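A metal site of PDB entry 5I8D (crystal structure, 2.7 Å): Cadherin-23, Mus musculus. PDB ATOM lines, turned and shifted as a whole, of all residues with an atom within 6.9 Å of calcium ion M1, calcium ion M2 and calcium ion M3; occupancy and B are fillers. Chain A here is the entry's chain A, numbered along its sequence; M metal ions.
The guanidinium group (NH2) of Arg 187 lies close to the side-chain carboxylate (OE1) of Glu 188 (3.0 Å). The side-chain carboxylate (OD1) of Asp 219 lies close to the guanidinium group (NE) of Arg 187. ND1 of His 323 lies within hydrogen-bond range of O of Asp 222 (2.8 Å). N of Asp 315 is in hydrogen-bond range of O of Ser 324 (2.8 Å). OD1 of Asp 315 lies close to N of Ala 317. The side-chain carboxylate of Asp 222 lies close to the side-chain amide nitrogen of Asn 134. The side-chain carboxylate of Asp 219 sits close to the backbone NH of Leu 256. The backbone carbonyl oxygen (O) of Asn 221 is in hydrogen-bond range of the backbone NH (N) of Asp 319.
Four residues have an atom within 4 Å of calcium ion M1: Glu 133, Asp 186, Glu 188 and Asp 222.
Of the 27 residues printed, 6 come within 4 Å of calcium ion M2. Along chain A the residues within 4 Å of calcium ion M2 span positions 133 to 255. The nearest printed residue that does not touch calcium ion M2 is Arg 187 (4.3 Å).
Within 4 Å of calcium ion M3: Asn 221, Ser 223, Asp 253, Asp 255 and Asp 315.
Calcium ion M1 is bound by the side-chain carboxylate (OE1) of Glu 133 (1.9 Å), the side-chain carboxylate (OD1) of Asp 186 (2.3 Å), the side-chain carboxylate (OE2) of Glu 188 (2.5 Å), the side-chain carboxylate (OD1) of Asp 222 (2.6 Å) and the side-chain carboxylate (OD2) of Asp 222 (2.7 Å). Calcium ion M1 has five donor atoms within binding distance.
Calcium ion M2 is bound by O of Ile 220 (2.3 Å). OD1 of Asp 219 binds calcium ion M2, 2.3 Å away. OE2 of Glu 188 binds calcium ion M2 (2.4 Å). The side-chain carboxylate (OD1) of Asp 255 binds calcium ion M2 (2.4 Å). OE2 of Glu 133 binds calcium ion M2 (2.6 Å). The side-chain carboxylate (OD1) of Asp 222 is bound to calcium ion M2, at 2.7 Å. OE1 of Glu 188 is bound to calcium ion M2 (2.7 Å).
Calcium ion M3 is bound by the side-chain carboxylate (OD2) of Asp 315 (2.2 Å), the backbone carbonyl oxygen (O) of Ser 223 (2.2 Å), the side-chain carboxylate (OD1) of Asp 253 (2.4 Å), the side-chain carboxylate (OD2) of Asp 255 (2.5 Å), the side-chain amide oxygen (OD1) of Asn 221 (2.6 Å) and the side-chain carboxylate (OD2) of Asp 253 (2.8 Å).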
ATOM      1  N   GLU A 133      -8.722  16.553  21.224  1.00  0.00           N
ATOM      2  CA  GLU A 133      -9.178  15.184  21.461  1.00  0.00           C
ATOM      3  C   GLU A 133     -10.385  15.072  22.422  1.00  0.00           C
ATOM      4  O   GLU A 133     -10.626  15.973  23.226  1.00  0.00           O
ATOM      5  CB  GLU A 133      -7.943  14.422  21.987  1.00  0.00           C
ATOM      6  CG  GLU A 133      -8.155  13.038  22.550  1.00  0.00           C
ATOM      7  CD  GLU A 133      -6.856  12.438  23.076  1.00  0.00           C
ATOM      8  OE1 GLU A 133      -6.926  11.244  23.452  1.00  0.00           O
ATOM      9  OE2 GLU A 133      -5.798  13.144  23.145  1.00  0.00           O
ATOM     10  N   ASN A 134     -11.145  13.958  22.321  1.00  0.00           N
ATOM     11  CA  ASN A 134     -12.343  13.719  23.203  1.00  0.00           C
ATOM     12  C   ASN A 134     -13.394  14.833  23.176  1.00  0.00           C
ATOM     13  O   ASN A 134     -13.728  15.421  24.188  1.00  0.00           O
ATOM     14  CB  ASN A 134     -11.950  13.520  24.679  1.00  0.00           C
ATOM     15  CG  ASN A 134     -10.998  12.390  24.875  1.00  0.00           C
ATOM     16  OD1 ASN A 134     -11.223  11.300  24.386  1.00  0.00           O
ATOM     17  ND2 ASN A 134      -9.924  12.638  25.610  1.00  0.00           N
ATOM     18  N   ILE A 185     -13.178  10.636  19.163  1.00  0.00           N
ATOM     19  CA  ILE A 185     -11.991  11.261  18.539  1.00  0.00           C
ATOM     20  C   ILE A 185     -10.808  11.141  19.480  1.00  0.00           C
ATOM     21  O   ILE A 185     -10.623  11.982  20.394  1.00  0.00           O
ATOM     22  CB  ILE A 185     -12.241  12.749  18.208  1.00  0.00           C
ATOM     23  CG1 ILE A 185     -13.384  12.892  17.201  1.00  0.00           C
ATOM     24  CG2 ILE A 185     -10.971  13.450  17.708  1.00  0.00           C
ATOM     25  CD1 ILE A 185     -13.191  12.162  15.885  1.00  0.00           C
ATOM     26  N   ASP A 186     -10.022  10.089  19.246  1.00  0.00           N
ATOM     27  CA  ASP A 186      -8.838   9.740  20.043  1.00  0.00           C
ATOM     28  C   ASP A 186      -7.530   9.967  19.287  1.00  0.00           C
ATOM     29  O   ASP A 186      -7.186   9.208  18.363  1.00  0.00           O
ATOM     30  CB  ASP A 186      -8.924   8.277  20.467  1.00  0.00           C
ATOM     31  CG  ASP A 186      -7.829   7.873  21.448  1.00  0.00           C
ATOM     32  OD1 ASP A 186      -7.152   8.759  22.001  1.00  0.00           O
ATOM     33  OD2 ASP A 186      -7.649   6.662  21.673  1.00  0.00           O
ATOM     34  N   ARG A 187      -6.786  10.979  19.707  1.00  0.00           N
ATOM     35  CA  ARG A 187      -5.443  11.256  19.164  1.00  0.00           C
ATOM     36  C   ARG A 187      -4.481  10.069  19.204  1.00  0.00           C
ATOM     37  O   ARG A 187      -3.549  10.007  18.379  1.00  0.00           O
ATOM     38  CB  ARG A 187      -4.784  12.414  19.905  1.00  0.00           C
ATOM     39  CG  ARG A 187      -3.740  13.126  19.056  1.00  0.00           C
ATOM     40  CD  ARG A 187      -2.730  13.851  19.901  1.00  0.00           C
ATOM     41  NE  ARG A 187      -1.896  12.901  20.638  1.00  0.00           N
ATOM     42  CZ  ARG A 187      -0.790  12.303  20.191  1.00  0.00           C
ATOM     43  NH1 ARG A 187      -0.298  12.546  18.956  1.00  0.00           N
ATOM     44  NH2 ARG A 187      -0.160  11.457  20.992  1.00  0.00           N
ATOM     45  N   GLU A 188      -4.679   9.162  20.158  1.00  0.00           N
ATOM     46  CA  GLU A 188      -3.887   7.924  20.251  1.00  0.00           C
ATOM     47  C   GLU A 188      -4.293   6.877  19.201  1.00  0.00           C
ATOM     48  O   GLU A 188      -3.492   6.012  18.860  1.00  0.00           O
ATOM     49  CB  GLU A 188      -3.922   7.329  21.675  1.00  0.00           C
ATOM     50  CG  GLU A 188      -2.999   8.019  22.681  1.00  0.00           C
ATOM     51  CD  GLU A 188      -3.310   9.498  22.914  1.00  0.00           C
ATOM     52  OE1 GLU A 188      -2.457  10.373  22.583  1.00  0.00           O
ATOM     53  OE2 GLU A 188      -4.417   9.802  23.458  1.00  0.00           O
ATOM     54  N   GLU A 189      -5.531   6.966  18.710  1.00  0.00           N
ATOM     55  CA  GLU A 189      -6.019   6.147  17.574  1.00  0.00           C
ATOM     56  C   GLU A 189      -5.635   6.814  16.258  1.00  0.00           C
ATOM     57  O   GLU A 189      -5.124   6.147  15.371  1.00  0.00           O
ATOM     58  CB  GLU A 189      -7.542   5.913  17.634  1.00  0.00           C
ATOM     59  CG  GLU A 189      -8.136   5.251  16.397  1.00  0.00           C
ATOM     60  CD  GLU A 189      -9.494   4.615  16.677  1.00  0.00           C
ATOM     61  OE1 GLU A 189      -9.636   3.402  16.397  1.00  0.00           O
ATOM     62  OE2 GLU A 189     -10.406   5.322  17.155  1.00  0.00           O
ATOM     63  N   ASP A 218      -5.297  17.612  18.493  1.00  0.00           N
ATOM     64  CA  ASP A 218      -4.457  18.075  19.613  1.00  0.00           C
ATOM     65  C   ASP A 218      -4.591  17.105  20.783  1.00  0.00           C
ATOM     66  O   ASP A 218      -5.572  16.367  20.883  1.00  0.00           O
ATOM     67  CB  ASP A 218      -4.775  19.525  20.000  1.00  0.00           C
ATOM     68  CG  ASP A 218      -4.115  20.550  19.067  1.00  0.00           C
ATOM     69  OD1 ASP A 218      -3.507  20.134  18.048  1.00  0.00           O
ATOM     70  OD2 ASP A 218      -4.203  21.764  19.336  1.00  0.00           O
ATOM     71  N   ASP A 219      -3.585  17.095  21.646  1.00  0.00           N
ATOM     72  CA  ASP A 219      -3.446  16.086  22.693  1.00  0.00           C
ATOM     73  C   ASP A 219      -3.942  16.582  24.033  1.00  0.00           C
ATOM     74  O   ASP A 219      -3.567  17.664  24.475  1.00  0.00           O
ATOM     75  CB  ASP A 219      -1.978  15.700  22.854  1.00  0.00           C
ATOM     76  CG  ASP A 219      -1.772  14.625  23.900  1.00  0.00           C
ATOM     77  OD1 ASP A 219      -2.394  13.548  23.758  1.00  0.00           O
ATOM     78  OD2 ASP A 219      -1.001  14.862  24.845  1.00  0.00           O
ATOM     79  N   ILE A 220      -4.777  15.763  24.681  1.00  0.00           N
ATOM     80  CA  ILE A 220      -4.927  15.793  26.113  1.00  0.00           C
ATOM     81  C   ILE A 220      -4.115  14.581  26.568  1.00  0.00           C
ATOM     82  O   ILE A 220      -4.152  13.536  25.922  1.00  0.00           O
ATOM     83  CB  ILE A 220      -6.407  15.606  26.537  1.00  0.00           C
ATOM     84  CG1 ILE A 220      -7.270  16.774  26.050  1.00  0.00           C
ATOM     85  CG2 ILE A 220      -6.531  15.503  28.060  1.00  0.00           C
ATOM     86  CD1 ILE A 220      -8.766  16.476  26.045  1.00  0.00           C
ATOM     87  N   ASN A 221      -3.367  14.726  27.667  1.00  0.00           N
ATOM     88  CA  ASN A 221      -2.669  13.579  28.289  1.00  0.00           C
ATOM     89  C   ASN A 221      -3.665  12.706  29.075  1.00  0.00           C
ATOM     90  O   ASN A 221      -3.872  12.902  30.292  1.00  0.00           O
ATOM     91  CB  ASN A 221      -1.519  14.055  29.176  1.00  0.00           C
ATOM     92  CG  ASN A 221      -0.638  12.895  29.630  1.00  0.00           C
ATOM     93  OD1 ASN A 221      -1.121  11.858  30.095  1.00  0.00           O
ATOM     94  ND2 ASN A 221       0.681  13.066  29.494  1.00  0.00           N
ATOM     95  N   ASP A 222      -4.242  11.730  28.373  1.00  0.00           N
ATOM     96  CA  ASP A 222      -5.366  10.976  28.887  1.00  0.00           C
ATOM     97  C   ASP A 222      -5.252   9.466  28.733  1.00  0.00           C
ATOM     98  O   ASP A 222      -6.237   8.757  28.918  1.00  0.00           O
ATOM     99  CB  ASP A 222      -6.625  11.444  28.160  1.00  0.00           C
ATOM    100  CG  ASP A 222      -6.651  11.043  26.709  1.00  0.00           C
ATOM    101  OD1 ASP A 222      -5.587  10.735  26.115  1.00  0.00           O
ATOM    102  OD2 ASP A 222      -7.757  11.037  26.145  1.00  0.00           O
ATOM    103  N   SER A 223      -4.061   8.971  28.424  1.00  0.00           N
ATOM    104  CA  SER A 223      -3.854   7.569  28.125  1.00  0.00           C
ATOM    105  C   SER A 223      -2.940   6.997  29.205  1.00  0.00           C
ATOM    106  O   SER A 223      -1.860   7.592  29.478  1.00  0.00           O
ATOM    107  CB  SER A 223      -3.193   7.444  26.769  1.00  0.00           C
ATOM    108  OG  SER A 223      -3.339   6.137  26.280  1.00  0.00           O
ATOM    109  N   ARG A 224      -3.359   5.903  29.856  1.00  0.00           N
ATOM    110  CA  ARG A 224      -2.573   5.360  30.985  1.00  0.00           C
ATOM    111  C   ARG A 224      -1.301   4.655  30.517  1.00  0.00           C
ATOM    112  O   ARG A 224      -1.287   4.032  29.447  1.00  0.00           O
ATOM    113  CB  ARG A 224      -3.419   4.454  31.920  1.00  0.00           C
ATOM    114  CG  ARG A 224      -3.845   3.115  31.330  1.00  0.00           C
ATOM    115  CD  ARG A 224      -4.460   2.177  32.372  1.00  0.00           C
ATOM    116  NE  ARG A 224      -5.856   2.503  32.677  1.00  0.00           N
ATOM    117  CZ  ARG A 224      -6.280   3.235  33.710  1.00  0.00           C
ATOM    118  NH1 ARG A 224      -5.413   3.778  34.569  1.00  0.00           N
ATOM    119  NH2 ARG A 224      -7.589   3.434  33.878  1.00  0.00           N
ATOM    120  N   PRO A 225      -0.217   4.739  31.310  1.00  0.00           N
ATOM    121  CA  PRO A 225       0.983   4.029  30.970  1.00  0.00           C
ATOM    122  C   PRO A 225       0.769   2.535  31.087  1.00  0.00           C
ATOM    123  O   PRO A 225       0.080   2.054  32.012  1.00  0.00           O
ATOM    124  CB  PRO A 225       2.000   4.520  32.001  1.00  0.00           C
ATOM    125  CG  PRO A 225       1.207   4.978  33.143  1.00  0.00           C
ATOM    126  CD  PRO A 225      -0.059   5.511  32.557  1.00  0.00           C
ATOM    127  N   ASP A 253       3.903   5.003  27.267  1.00  0.00           N
ATOM    128  CA  ASP A 253       2.770   5.909  27.396  1.00  0.00           C
ATOM    129  C   ASP A 253       2.621   6.585  26.049  1.00  0.00           C
ATOM    130  O   ASP A 253       3.559   7.215  25.583  1.00  0.00           O
ATOM    131  CB  ASP A 253       3.031   6.935  28.487  1.00  0.00           C
ATOM    132  CG  ASP A 253       1.755   7.563  29.047  1.00  0.00           C
ATOM    133  OD1 ASP A 253       1.187   8.502  28.452  1.00  0.00           O
ATOM    134  OD2 ASP A 253       1.305   7.151  30.142  1.00  0.00           O
ATOM    135  N   LEU A 254       1.452   6.454  25.438  1.00  0.00           N
ATOM    136  CA  LEU A 254       1.254   6.917  24.063  1.00  0.00           C
ATOM    137  C   LEU A 254       0.873   8.389  23.920  1.00  0.00           C
ATOM    138  O   LEU A 254       0.649   8.866  22.807  1.00  0.00           O
ATOM    139  CB  LEU A 254       0.202   6.055  23.385  1.00  0.00           C
ATOM    140  CG  LEU A 254       0.513   4.562  23.354  1.00  0.00           C
ATOM    141  CD1 LEU A 254      -0.729   3.784  22.955  1.00  0.00           C
ATOM    142  CD2 LEU A 254       1.663   4.284  22.420  1.00  0.00           C
ATOM    143  N   ASP A 255       0.815   9.119  25.034  1.00  0.00           N
ATOM    144  CA  ASP A 255       0.565  10.562  25.000  1.00  0.00           C
ATOM    145  C   ASP A 255       1.804  11.325  24.538  1.00  0.00           C
ATOM    146  O   ASP A 255       2.876  10.744  24.334  1.00  0.00           O
ATOM    147  CB  ASP A 255       0.083  11.045  26.382  1.00  0.00           C
ATOM    148  CG  ASP A 255      -1.350  10.640  26.682  1.00  0.00           C
ATOM    149  OD1 ASP A 255      -2.229  10.919  25.837  1.00  0.00           O
ATOM    150  OD2 ASP A 255      -1.608  10.056  27.769  1.00  0.00           O
ATOM    151  N   LEU A 256       1.646  12.632  24.389  1.00  0.00           N
ATOM    152  CA  LEU A 256       2.616  13.481  23.716  1.00  0.00           C
ATOM    153  C   LEU A 256       3.872  13.783  24.531  1.00  0.00           C
ATOM    154  O   LEU A 256       4.953  13.817  23.977  1.00  0.00           O
ATOM    155  CB  LEU A 256       1.929  14.769  23.257  1.00  0.00           C
ATOM    156  CG  LEU A 256       2.456  15.487  21.999  1.00  0.00           C
ATOM    157  CD1 LEU A 256       2.542  14.589  20.776  1.00  0.00           C
ATOM    158  CD2 LEU A 256       1.552  16.680  21.720  1.00  0.00           C
ATOM    159  N   PRO A 258       4.873  12.479  28.144  1.00  0.00           N
ATOM    160  CA  PRO A 258       4.709  11.795  29.409  1.00  0.00           C
ATOM    161  C   PRO A 258       5.917  11.928  30.315  1.00  0.00           C
ATOM    162  O   PRO A 258       7.041  11.923  29.835  1.00  0.00           O
ATOM    163  CB  PRO A 258       4.509  10.335  29.011  1.00  0.00           C
ATOM    164  CG  PRO A 258       5.132  10.202  27.676  1.00  0.00           C
ATOM    165  CD  PRO A 258       5.205  11.554  27.046  1.00  0.00           C
ATOM    166  N   LEU A 260       6.932   9.651  33.117  1.00  0.00           N
ATOM    167  CA  LEU A 260       6.750   8.390  33.810  1.00  0.00           C
ATOM    168  C   LEU A 260       7.674   8.239  35.013  1.00  0.00           C
ATOM    169  O   LEU A 260       8.883   8.360  34.877  1.00  0.00           O
ATOM    170  CB  LEU A 260       7.027   7.225  32.852  1.00  0.00           C
ATOM    171  CG  LEU A 260       6.246   7.124  31.540  1.00  0.00           C
ATOM    172  CD1 LEU A 260       6.183   5.675  31.089  1.00  0.00           C
ATOM    173  CD2 LEU A 260       4.838   7.639  31.655  1.00  0.00           C
ATOM    174  N   ASP A 315       2.173   8.505  35.306  1.00  0.00           N
ATOM    175  CA  ASP A 315       2.443   9.596  34.371  1.00  0.00           C
ATOM    176  C   ASP A 315       2.200  10.976  35.037  1.00  0.00           C
ATOM    177  O   ASP A 315       1.087  11.492  35.059  1.00  0.00           O
ATOM    178  CB  ASP A 315       1.570   9.420  33.123  1.00  0.00           C
ATOM    179  CG  ASP A 315       1.966  10.333  31.962  1.00  0.00           C
ATOM    180  OD1 ASP A 315       2.861  11.184  32.136  1.00  0.00           O
ATOM    181  OD2 ASP A 315       1.370  10.174  30.860  1.00  0.00           O
ATOM    182  N   ALA A 317       2.683  13.908  34.115  1.00  0.00           N
ATOM    183  CA  ALA A 317       2.077  14.877  33.209  1.00  0.00           C
ATOM    184  C   ALA A 317       0.586  14.657  32.982  1.00  0.00           C
ATOM    185  O   ALA A 317      -0.046  15.471  32.327  1.00  0.00           O
ATOM    186  CB  ALA A 317       2.812  14.839  31.863  1.00  0.00           C
ATOM    187  N   SER A 318       0.018  13.579  33.521  1.00  0.00           N
ATOM    188  CA  SER A 318      -1.386  13.201  33.254  1.00  0.00           C
ATOM    189  C   SER A 318      -2.421  14.296  33.520  1.00  0.00           C
ATOM    190  O   SER A 318      -2.377  14.948  34.557  1.00  0.00           O
ATOM    191  CB  SER A 318      -1.762  11.981  34.093  1.00  0.00           C
ATOM    192  OG  SER A 318      -3.187  11.688  33.960  1.00  0.00           O
ATOM    193  N   ASP A 319      -3.366  14.456  32.572  1.00  0.00           N
ATOM    194  CA  ASP A 319      -4.458  15.446  32.718  1.00  0.00           C
ATOM    195  C   ASP A 319      -5.733  14.854  33.348  1.00  0.00           C
ATOM    196  O   ASP A 319      -6.637  15.609  33.714  1.00  0.00           O
ATOM    197  CB  ASP A 319      -4.776  16.085  31.367  1.00  0.00           C
ATOM    198  CG  ASP A 319      -3.669  17.020  30.859  1.00  0.00           C
ATOM    199  OD1 ASP A 319      -3.274  17.959  31.587  1.00  0.00           O
ATOM    200  OD2 ASP A 319      -3.217  16.835  29.708  1.00  0.00           O
ATOM    201  N   HIS A 323      -6.476   8.082  34.407  1.00  0.00           N
ATOM    202  CA  HIS A 323      -5.604   7.487  33.389  1.00  0.00           C
ATOM    203  C   HIS A 323      -4.132   7.885  33.608  1.00  0.00           C
ATOM    204  O   HIS A 323      -3.386   8.216  32.647  1.00  0.00           O
ATOM    205  CB  HIS A 323      -6.103   7.860  31.985  1.00  0.00           C
ATOM    206  CG  HIS A 323      -7.490   7.371  31.686  1.00  0.00           C
ATOM    207  ND1 HIS A 323      -8.276   7.938  30.699  1.00  0.00           N
ATOM    208  CD2 HIS A 323      -8.231   6.379  32.228  1.00  0.00           C
ATOM    209  CE1 HIS A 323      -9.442   7.307  30.666  1.00  0.00           C
ATOM    210  NE2 HIS A 323      -9.435   6.358  31.573  1.00  0.00           N
ATOM    211  N   SER A 324      -3.717   7.865  34.882  1.00  0.00           N
ATOM    212  CA  SER A 324      -2.370   8.280  35.301  1.00  0.00           C
ATOM    213  C   SER A 324      -1.510   7.142  35.808  1.00  0.00           C
ATOM    214  O   SER A 324      -0.298   7.252  35.758  1.00  0.00           O
ATOM    215  CB  SER A 324      -2.463   9.363  36.391  1.00  0.00           C
ATOM    216  OG  SER A 324      -3.326   8.991  37.447  1.00  0.00           O
HETATM  217 CA    CA M   1      -6.772   9.485  24.147  1.00  0.00          CA
HETATM  218 CA    CA M   2      -3.870  11.897  24.375  1.00  0.00          CA
HETATM  219 CA    CA M   3      -0.482   9.309  29.931  1.00  0.00          CA
